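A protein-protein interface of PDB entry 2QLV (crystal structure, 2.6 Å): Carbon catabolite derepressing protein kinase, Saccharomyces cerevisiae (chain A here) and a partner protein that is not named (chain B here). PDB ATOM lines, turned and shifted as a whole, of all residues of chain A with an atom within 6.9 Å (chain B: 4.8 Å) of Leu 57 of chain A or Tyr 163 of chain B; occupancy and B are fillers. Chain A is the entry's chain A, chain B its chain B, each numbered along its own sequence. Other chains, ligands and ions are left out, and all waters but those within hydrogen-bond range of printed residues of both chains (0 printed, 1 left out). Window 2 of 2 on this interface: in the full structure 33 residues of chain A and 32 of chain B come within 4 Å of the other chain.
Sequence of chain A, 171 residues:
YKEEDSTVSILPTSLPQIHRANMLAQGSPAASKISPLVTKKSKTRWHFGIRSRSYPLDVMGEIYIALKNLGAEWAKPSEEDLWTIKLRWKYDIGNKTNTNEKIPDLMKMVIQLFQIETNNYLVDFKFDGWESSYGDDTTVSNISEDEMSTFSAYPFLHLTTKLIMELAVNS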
ATOM      1  N   SER A  54       2.847 -25.944 -14.642  1.00  0.00           N
ATOM      2  CA  SER A  54       3.554 -25.701 -13.395  1.00  0.00           C
ATOM      3  C   SER A  54       2.615 -25.926 -12.224  1.00  0.00           C
ATOM      4  O   SER A  54       1.428 -26.151 -12.422  1.00  0.00           O
ATOM      5  CB  SER A  54       4.097 -24.277 -13.377  1.00  0.00           C
ATOM      6  OG  SER A  54       3.092 -23.361 -13.759  1.00  0.00           O
ATOM      7  N   TYR A  55       3.150 -25.868 -11.008  1.00  0.00           N
ATOM      8  CA  TYR A  55       2.352 -26.101  -9.806  1.00  0.00           C
ATOM      9  C   TYR A  55       1.193 -25.134  -9.680  1.00  0.00           C
ATOM     10  O   TYR A  55       1.366 -23.928  -9.818  1.00  0.00           O
ATOM     11  CB  TYR A  55       3.219 -26.016  -8.544  1.00  0.00           C
ATOM     12  CG  TYR A  55       4.398 -26.965  -8.539  1.00  0.00           C
ATOM     13  CD1 TYR A  55       5.596 -26.619  -9.165  1.00  0.00           C
ATOM     14  CD2 TYR A  55       4.307 -28.221  -7.937  1.00  0.00           C
ATOM     15  CE1 TYR A  55       6.679 -27.497  -9.195  1.00  0.00           C
ATOM     16  CE2 TYR A  55       5.382 -29.108  -7.961  1.00  0.00           C
ATOM     17  CZ  TYR A  55       6.568 -28.738  -8.593  1.00  0.00           C
ATOM     18  OH  TYR A  55       7.639 -29.603  -8.625  1.00  0.00           O
ATOM     19  N   PRO A  56      -0.011 -25.661  -9.400  1.00  0.00           N
ATOM     20  CA  PRO A  56      -1.250 -24.891  -9.242  1.00  0.00           C
ATOM     21  C   PRO A  56      -1.279 -23.861  -8.107  1.00  0.00           C
ATOM     22  O   PRO A  56      -2.247 -23.113  -7.966  1.00  0.00           O
ATOM     23  CB  PRO A  56      -2.313 -25.982  -9.093  1.00  0.00           C
ATOM     24  CG  PRO A  56      -1.564 -27.099  -8.469  1.00  0.00           C
ATOM     25  CD  PRO A  56      -0.274 -27.100  -9.238  1.00  0.00           C
ATOM     26  N   LEU A  57      -0.225 -23.818  -7.299  1.00  0.00           N
ATOM     27  CA  LEU A  57      -0.153 -22.840  -6.217  1.00  0.00           C
ATOM     28  C   LEU A  57       0.613 -21.621  -6.709  1.00  0.00           C
ATOM     29  O   LEU A  57       0.255 -20.478  -6.402  1.00  0.00           O
ATOM     30  CB  LEU A  57       0.559 -23.415  -4.987  1.00  0.00           C
ATOM     31  CG  LEU A  57      -0.211 -24.321  -4.028  1.00  0.00           C
ATOM     32  CD1 LEU A  57       0.665 -24.577  -2.809  1.00  0.00           C
ATOM     33  CD2 LEU A  57      -1.523 -23.668  -3.608  1.00  0.00           C
ATOM     34  N   ASP A  58       1.669 -21.872  -7.478  1.00  0.00           N
ATOM     35  CA  ASP A  58       2.489 -20.795  -8.020  1.00  0.00           C
ATOM     36  C   ASP A  58       1.761 -20.078  -9.148  1.00  0.00           C
ATOM     37  O   ASP A  58       2.127 -18.962  -9.524  1.00  0.00           O
ATOM     38  CB  ASP A  58       3.826 -21.349  -8.513  1.00  0.00           C
ATOM     39  CG  ASP A  58       4.686 -21.880  -7.381  1.00  0.00           C
ATOM     40  OD1 ASP A  58       5.155 -21.060  -6.553  1.00  0.00           O
ATOM     41  OD2 ASP A  58       4.878 -23.117  -7.318  1.00  0.00           O
ATOM     42  N   VAL A  59       0.731 -20.734  -9.679  1.00  0.00           N
ATOM     43  CA  VAL A  59      -0.102 -20.181 -10.744  1.00  0.00           C
ATOM     44  C   VAL A  59      -1.166 -19.305 -10.083  1.00  0.00           C
ATOM     45  O   VAL A  59      -1.332 -18.130 -10.412  1.00  0.00           O
ATOM     46  CB  VAL A  59      -0.801 -21.313 -11.553  1.00  0.00           C
ATOM     47  CG1 VAL A  59      -1.975 -20.758 -12.347  1.00  0.00           C
ATOM     48  CG2 VAL A  59       0.197 -21.965 -12.493  1.00  0.00           C
ATOM     49  N   MET A  60      -1.872 -19.907  -9.135  1.00  0.00           N
ATOM     50  CA  MET A  60      -2.922 -19.238  -8.382  1.00  0.00           C
ATOM     51  C   MET A  60      -2.352 -18.007  -7.666  1.00  0.00           C
ATOM     52  O   MET A  60      -3.035 -16.996  -7.490  1.00  0.00           O
ATOM     53  CB  MET A  60      -3.481 -20.217  -7.353  1.00  0.00           C
ATOM     54  CG  MET A  60      -4.944 -20.052  -7.041  1.00  0.00           C
ATOM     55  SD  MET A  60      -5.966 -20.619  -8.402  1.00  0.00           S
ATOM     56  CE  MET A  60      -6.731 -19.072  -8.878  1.00  0.00           C
ATOM     57  N   GLY A  61      -1.092 -18.102  -7.255  1.00  0.00           N
ATOM     58  CA  GLY A  61      -0.471 -17.001  -6.553  1.00  0.00           C
ATOM     59  C   GLY A  61      -0.177 -15.838  -7.465  1.00  0.00           C
ATOM     60  O   GLY A  61      -0.524 -14.694  -7.179  1.00  0.00           O
ATOM     61  N   GLU A  62       0.468 -16.123  -8.584  1.00  0.00           N
ATOM     62  CA  GLU A  62       0.793 -15.057  -9.504  1.00  0.00           C
ATOM     63  C   GLU A  62      -0.473 -14.363 -10.006  1.00  0.00           C
ATOM     64  O   GLU A  62      -0.449 -13.181 -10.323  1.00  0.00           O
ATOM     65  CB  GLU A  62       1.626 -15.599 -10.665  1.00  0.00           C
ATOM     66  CG  GLU A  62       2.789 -14.685 -11.017  1.00  0.00           C
ATOM     67  CD  GLU A  62       3.895 -15.398 -11.770  1.00  0.00           C
ATOM     68  OE1 GLU A  62       3.732 -15.643 -12.986  1.00  0.00           O
ATOM     69  OE2 GLU A  62       4.929 -15.722 -11.140  1.00  0.00           O
ATOM     70  N   ILE A  63      -1.581 -15.091 -10.068  1.00  0.00           N
ATOM     71  CA  ILE A  63      -2.824 -14.488 -10.510  1.00  0.00           C
ATOM     72  C   ILE A  63      -3.229 -13.441  -9.488  1.00  0.00           C
ATOM     73  O   ILE A  63      -3.513 -12.304  -9.852  1.00  0.00           O
ATOM     74  CB  ILE A  63      -3.966 -15.531 -10.657  1.00  0.00           C
ATOM     75  CG1 ILE A  63      -3.647 -16.489 -11.813  1.00  0.00           C
ATOM     76  CG2 ILE A  63      -5.302 -14.819 -10.897  1.00  0.00           C
ATOM     77  CD1 ILE A  63      -4.636 -17.614 -11.971  1.00  0.00           C
ATOM     78  N   TRP A  83      -9.928 -22.974  -5.694  1.00  0.00           N
ATOM     79  CA  TRP A  83      -9.224 -22.566  -6.888  1.00  0.00           C
ATOM     80  C   TRP A  83     -10.097 -21.637  -7.709  1.00  0.00           C
ATOM     81  O   TRP A  83      -9.911 -21.485  -8.914  1.00  0.00           O
ATOM     82  CB  TRP A  83      -8.820 -23.798  -7.686  1.00  0.00           C
ATOM     83  CG  TRP A  83      -8.149 -24.831  -6.829  1.00  0.00           C
ATOM     84  CD1 TRP A  83      -8.758 -25.774  -6.057  1.00  0.00           C
ATOM     85  CD2 TRP A  83      -6.742 -24.973  -6.599  1.00  0.00           C
ATOM     86  NE1 TRP A  83      -7.821 -26.494  -5.360  1.00  0.00           N
ATOM     87  CE2 TRP A  83      -6.575 -26.022  -5.672  1.00  0.00           C
ATOM     88  CE3 TRP A  83      -5.606 -24.312  -7.084  1.00  0.00           C
ATOM     89  CZ2 TRP A  83      -5.316 -26.427  -5.218  1.00  0.00           C
ATOM     90  CZ3 TRP A  83      -4.353 -24.714  -6.633  1.00  0.00           C
ATOM     91  CH2 TRP A  83      -4.220 -25.762  -5.708  1.00  0.00           C
ATOM     92  N   LEU A 113      -9.603 -22.640 -11.851  1.00  0.00           N
ATOM     93  CA  LEU A 113      -8.425 -23.395 -12.222  1.00  0.00           C
ATOM     94  C   LEU A 113      -8.912 -24.795 -12.537  1.00  0.00           C
ATOM     95  O   LEU A 113      -9.842 -25.289 -11.893  1.00  0.00           O
ATOM     96  CB  LEU A 113      -7.413 -23.433 -11.083  1.00  0.00           C
ATOM     97  CG  LEU A 113      -6.068 -23.932 -11.601  1.00  0.00           C
ATOM     98  CD1 LEU A 113      -5.532 -22.925 -12.615  1.00  0.00           C
ATOM     99  CD2 LEU A 113      -5.097 -24.122 -10.453  1.00  0.00           C
ATOM    100  N   VAL B 152      -1.802 -19.105   1.647  1.00  0.00           N
ATOM    101  CA  VAL B 152      -1.594 -20.424   1.057  1.00  0.00           C
ATOM    102  C   VAL B 152      -1.005 -20.314  -0.341  1.00  0.00           C
ATOM    103  O   VAL B 152      -0.564 -21.306  -0.918  1.00  0.00           O
ATOM    104  CB  VAL B 152      -2.905 -21.203   0.961  1.00  0.00           C
ATOM    105  CG1 VAL B 152      -2.626 -22.632   0.525  1.00  0.00           C
ATOM    106  CG2 VAL B 152      -3.619 -21.168   2.309  1.00  0.00           C
ATOM    107  N   PHE B 153      -1.000 -19.103  -0.887  1.00  0.00           N
ATOM    108  CA  PHE B 153      -0.445 -18.876  -2.216  1.00  0.00           C
ATOM    109  C   PHE B 153       0.780 -17.972  -2.142  1.00  0.00           C
ATOM    110  O   PHE B 153       1.431 -17.716  -3.159  1.00  0.00           O
ATOM    111  CB  PHE B 153      -1.494 -18.248  -3.146  1.00  0.00           C
ATOM    112  CG  PHE B 153      -2.688 -19.131  -3.406  1.00  0.00           C
ATOM    113  CD1 PHE B 153      -3.971 -18.723  -3.017  1.00  0.00           C
ATOM    114  CD2 PHE B 153      -2.535 -20.362  -4.040  1.00  0.00           C
ATOM    115  CE1 PHE B 153      -5.091 -19.527  -3.258  1.00  0.00           C
ATOM    116  CE2 PHE B 153      -3.652 -21.177  -4.285  1.00  0.00           C
ATOM    117  CZ  PHE B 153      -4.935 -20.754  -3.891  1.00  0.00           C
ATOM    118  N   MET B 159       2.629 -23.230   2.545  1.00  0.00           N
ATOM    119  CA  MET B 159       2.648 -24.021   1.318  1.00  0.00           C
ATOM    120  C   MET B 159       3.206 -25.434   1.558  1.00  0.00           C
ATOM    121  O   MET B 159       2.639 -26.421   1.068  1.00  0.00           O
ATOM    122  CB  MET B 159       3.461 -23.293   0.239  1.00  0.00           C
ATOM    123  CG  MET B 159       2.848 -21.950  -0.149  1.00  0.00           C
ATOM    124  SD  MET B 159       3.735 -21.024  -1.420  1.00  0.00           S
ATOM    125  CE  MET B 159       2.690 -21.384  -2.903  1.00  0.00           C
ATOM    126  N   GLU B 160       4.299 -25.529   2.319  1.00  0.00           N
ATOM    127  CA  GLU B 160       4.909 -26.822   2.633  1.00  0.00           C
ATOM    128  C   GLU B 160       3.953 -27.674   3.449  1.00  0.00           C
ATOM    129  O   GLU B 160       4.101 -28.899   3.515  1.00  0.00           O
ATOM    130  CB  GLU B 160       6.208 -26.633   3.414  1.00  0.00           C
ATOM    131  CG  GLU B 160       7.286 -25.936   2.622  1.00  0.00           C
ATOM    132  CD  GLU B 160       7.466 -26.568   1.253  1.00  0.00           C
ATOM    133  OE1 GLU B 160       7.883 -27.749   1.206  1.00  0.00           O
ATOM    134  OE2 GLU B 160       7.177 -25.889   0.233  1.00  0.00           O
ATOM    135  N   ARG B 161       2.979 -27.020   4.076  1.00  0.00           N
ATOM    136  CA  ARG B 161       1.984 -27.716   4.882  1.00  0.00           C
ATOM    137  C   ARG B 161       0.917 -28.212   3.925  1.00  0.00           C
ATOM    138  O   ARG B 161       0.228 -29.193   4.194  1.00  0.00           O
ATOM    139  CB  ARG B 161       1.367 -26.762   5.904  1.00  0.00           C
ATOM    140  CG  ARG B 161       2.397 -26.007   6.705  1.00  0.00           C
ATOM    141  CD  ARG B 161       1.838 -24.719   7.296  1.00  0.00           C
ATOM    142  NE  ARG B 161       1.048 -24.936   8.503  1.00  0.00           N
ATOM    143  CZ  ARG B 161       0.673 -23.954   9.317  1.00  0.00           C
ATOM    144  NH1 ARG B 161       1.022 -22.698   9.037  1.00  0.00           N
ATOM    145  NH2 ARG B 161      -0.049 -24.223  10.408  1.00  0.00           N
ATOM    146  N   TYR B 162       0.779 -27.511   2.804  1.00  0.00           N
ATOM    147  CA  TYR B 162      -0.181 -27.902   1.794  1.00  0.00           C
ATOM    148  C   TYR B 162       0.284 -29.253   1.262  1.00  0.00           C
ATOM    149  O   TYR B 162      -0.427 -30.250   1.347  1.00  0.00           O
ATOM    150  CB  TYR B 162      -0.200 -26.891   0.643  1.00  0.00           C
ATOM    151  CG  TYR B 162      -1.095 -27.314  -0.509  1.00  0.00           C
ATOM    152  CD1 TYR B 162      -2.483 -27.265  -0.385  1.00  0.00           C
ATOM    153  CD2 TYR B 162      -0.555 -27.828  -1.691  1.00  0.00           C
ATOM    154  CE1 TYR B 162      -3.317 -27.718  -1.402  1.00  0.00           C
ATOM    155  CE2 TYR B 162      -1.378 -28.285  -2.712  1.00  0.00           C
ATOM    156  CZ  TYR B 162      -2.764 -28.230  -2.559  1.00  0.00           C
ATOM    157  OH  TYR B 162      -3.609 -28.707  -3.544  1.00  0.00           O
ATOM    158  N   TYR B 163       1.498 -29.272   0.722  1.00  0.00           N
ATOM    159  CA  TYR B 163       2.067 -30.483   0.163  1.00  0.00           C
ATOM    160  C   TYR B 163       2.131 -31.669   1.145  1.00  0.00           C
ATOM    161  O   TYR B 163       2.151 -32.826   0.724  1.00  0.00           O
ATOM    162  CB  TYR B 163       3.459 -30.181  -0.393  1.00  0.00           C
ATOM    163  CG  TYR B 163       3.471 -29.194  -1.551  1.00  0.00           C
ATOM    164  CD1 TYR B 163       3.236 -27.835  -1.346  1.00  0.00           C
ATOM    165  CD2 TYR B 163       3.736 -29.628  -2.855  1.00  0.00           C
ATOM    166  CE1 TYR B 163       3.271 -26.929  -2.409  1.00  0.00           C
ATOM    167  CE2 TYR B 163       3.768 -28.733  -3.929  1.00  0.00           C
ATOM    168  CZ  TYR B 163       3.537 -27.388  -3.703  1.00  0.00           C
ATOM    169  OH  TYR B 163       3.567 -26.512  -4.772  1.00  0.00           O
ATOM    170  N   TYR B 164       2.166 -31.383   2.444  1.00  0.00           N
ATOM    171  CA  TYR B 164       2.208 -32.427   3.470  1.00  0.00           C
ATOM    172  C   TYR B 164       0.854 -33.137   3.562  1.00  0.00           C
ATOM    173  O   TYR B 164       0.792 -34.370   3.567  1.00  0.00           O
ATOM    174  CB  TYR B 164       2.556 -31.809   4.827  1.00  0.00           C
ATOM    175  CG  TYR B 164       2.269 -32.695   6.029  1.00  0.00           C
ATOM    176  CD1 TYR B 164       3.054 -33.820   6.301  1.00  0.00           C
ATOM    177  CD2 TYR B 164       1.218 -32.397   6.903  1.00  0.00           C
ATOM    178  CE1 TYR B 164       2.803 -34.630   7.420  1.00  0.00           C
ATOM    179  CE2 TYR B 164       0.957 -33.198   8.023  1.00  0.00           C
ATOM    180  CZ  TYR B 164       1.755 -34.314   8.277  1.00  0.00           C
ATOM    181  OH  TYR B 164       1.515 -35.098   9.391  1.00  0.00           O
ATOM    182  N   THR B 165      -0.223 -32.352   3.651  1.00  0.00           N
ATOM    183  CA  THR B 165      -1.573 -32.907   3.723  1.00  0.00           C
ATOM    184  C   THR B 165      -2.007 -33.444   2.347  1.00  0.00           C
ATOM    185  O   THR B 165      -2.865 -34.324   2.246  1.00  0.00           O
ATOM    186  CB  THR B 165      -2.614 -31.846   4.197  1.00  0.00           C
ATOM    187  OG1 THR B 165      -2.410 -30.620   3.487  1.00  0.00           O
ATOM    188  CG2 THR B 165      -2.497 -31.587   5.697  1.00  0.00           C
ATOM    189  N   LEU B 166      -1.388 -32.917   1.294  1.00  0.00           N
ATOM    190  CA  LEU B 166      -1.692 -33.315  -0.076  1.00  0.00           C
ATOM    191  C   LEU B 166      -1.114 -34.670  -0.462  1.00  0.00           C
ATOM    192  O   LEU B 166      -1.833 -35.559  -0.934  1.00  0.00           O
ATOM    193  CB  LEU B 166      -1.166 -32.271  -1.064  1.00  0.00           C
ATOM    194  CG  LEU B 166      -1.166 -32.785  -2.508  1.00  0.00           C
ATOM    195  CD1 LEU B 166      -2.595 -33.101  -2.915  1.00  0.00           C
ATOM    196  CD2 LEU B 166      -0.538 -31.759  -3.448  1.00  0.00           C
ATOM    197  N   ASP B 167       0.192 -34.814  -0.288  1.00  0.00           N
ATOM    198  CA  ASP B 167       0.854 -36.061  -0.636  1.00  0.00           C
ATOM    199  C   ASP B 167       0.702 -37.111   0.457  1.00  0.00           C
ATOM    200  O   ASP B 167       1.525 -38.012   0.574  1.00  0.00           O
ATOM    201  CB  ASP B 167       2.342 -35.812  -0.932  1.00  0.00           C
ATOM    202  CG  ASP B 167       2.559 -34.890  -2.133  1.00  0.00           C
ATOM    203  OD1 ASP B 167       2.067 -35.220  -3.243  1.00  0.00           O
ATOM    204  OD2 ASP B 167       3.225 -33.837  -1.962  1.00  0.00           O
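N of Leu 113 of chain A is in hydrogen-bond range of O of Trp 83 of chain A, at 3.2 Å. The backbone carbonyl oxygen (O) of Tyr 162 of chain B lies within hydrogen-bond range of the side-chain hydroxyl (OG1) of Thr 165 of chain B (2.9 Å).
Tyr 55 of chain A touches Tyr 163 of chain B. Val 152 of chain B touches Leu 57 of chain A. CE2 of Phe 153 of chain B touches CD2 of Leu 57 of chain A, 3.3 Å away. CE of Met 159 of chain B touches CB of Leu 57 of chain A (3.6 Å). Leu 57 of chain A touches Tyr 162 of chain B (CD1 to CD2, 3.6 Å). Leu 57 of chain A touches Tyr 163 of chain B (CD1 to CE1, 3.5 Å). Met 60 of chain A touches Phe 153 of chain B. CB of Phe 153 of chain B touches CA of Gly 61 of chain A, 3.8 Å away. OH of Tyr 162 of chain B touches CZ2 of Trp 83 of chain A, 3.3 Å away.
Leu 57 of chain A touches five residues of chain B. Of the printed residues of chain B, Met 60 of chain A touches Phe 153 (3.2 Å). Of the printed residues of chain A, Phe 153 of chain B touches Leu 57, Met 60 and Gly 61. Tyr 163 of chain B touches two residues of chain A.
Hydrophobic or aromatic side chains of chain A that line the printed part of chain B: Tyr 55, Leu 57, Met 60 and Trp 83. Of the 11 printed residues of chain B, 5 touch a printed residue of chain A. Hydrophobic or aromatic side chains of chain B that line the printed part of chain A: Phe 153, Met 159, Tyr 162 and Tyr 163. Among the printed residues, 9 pairs touch across the chains.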
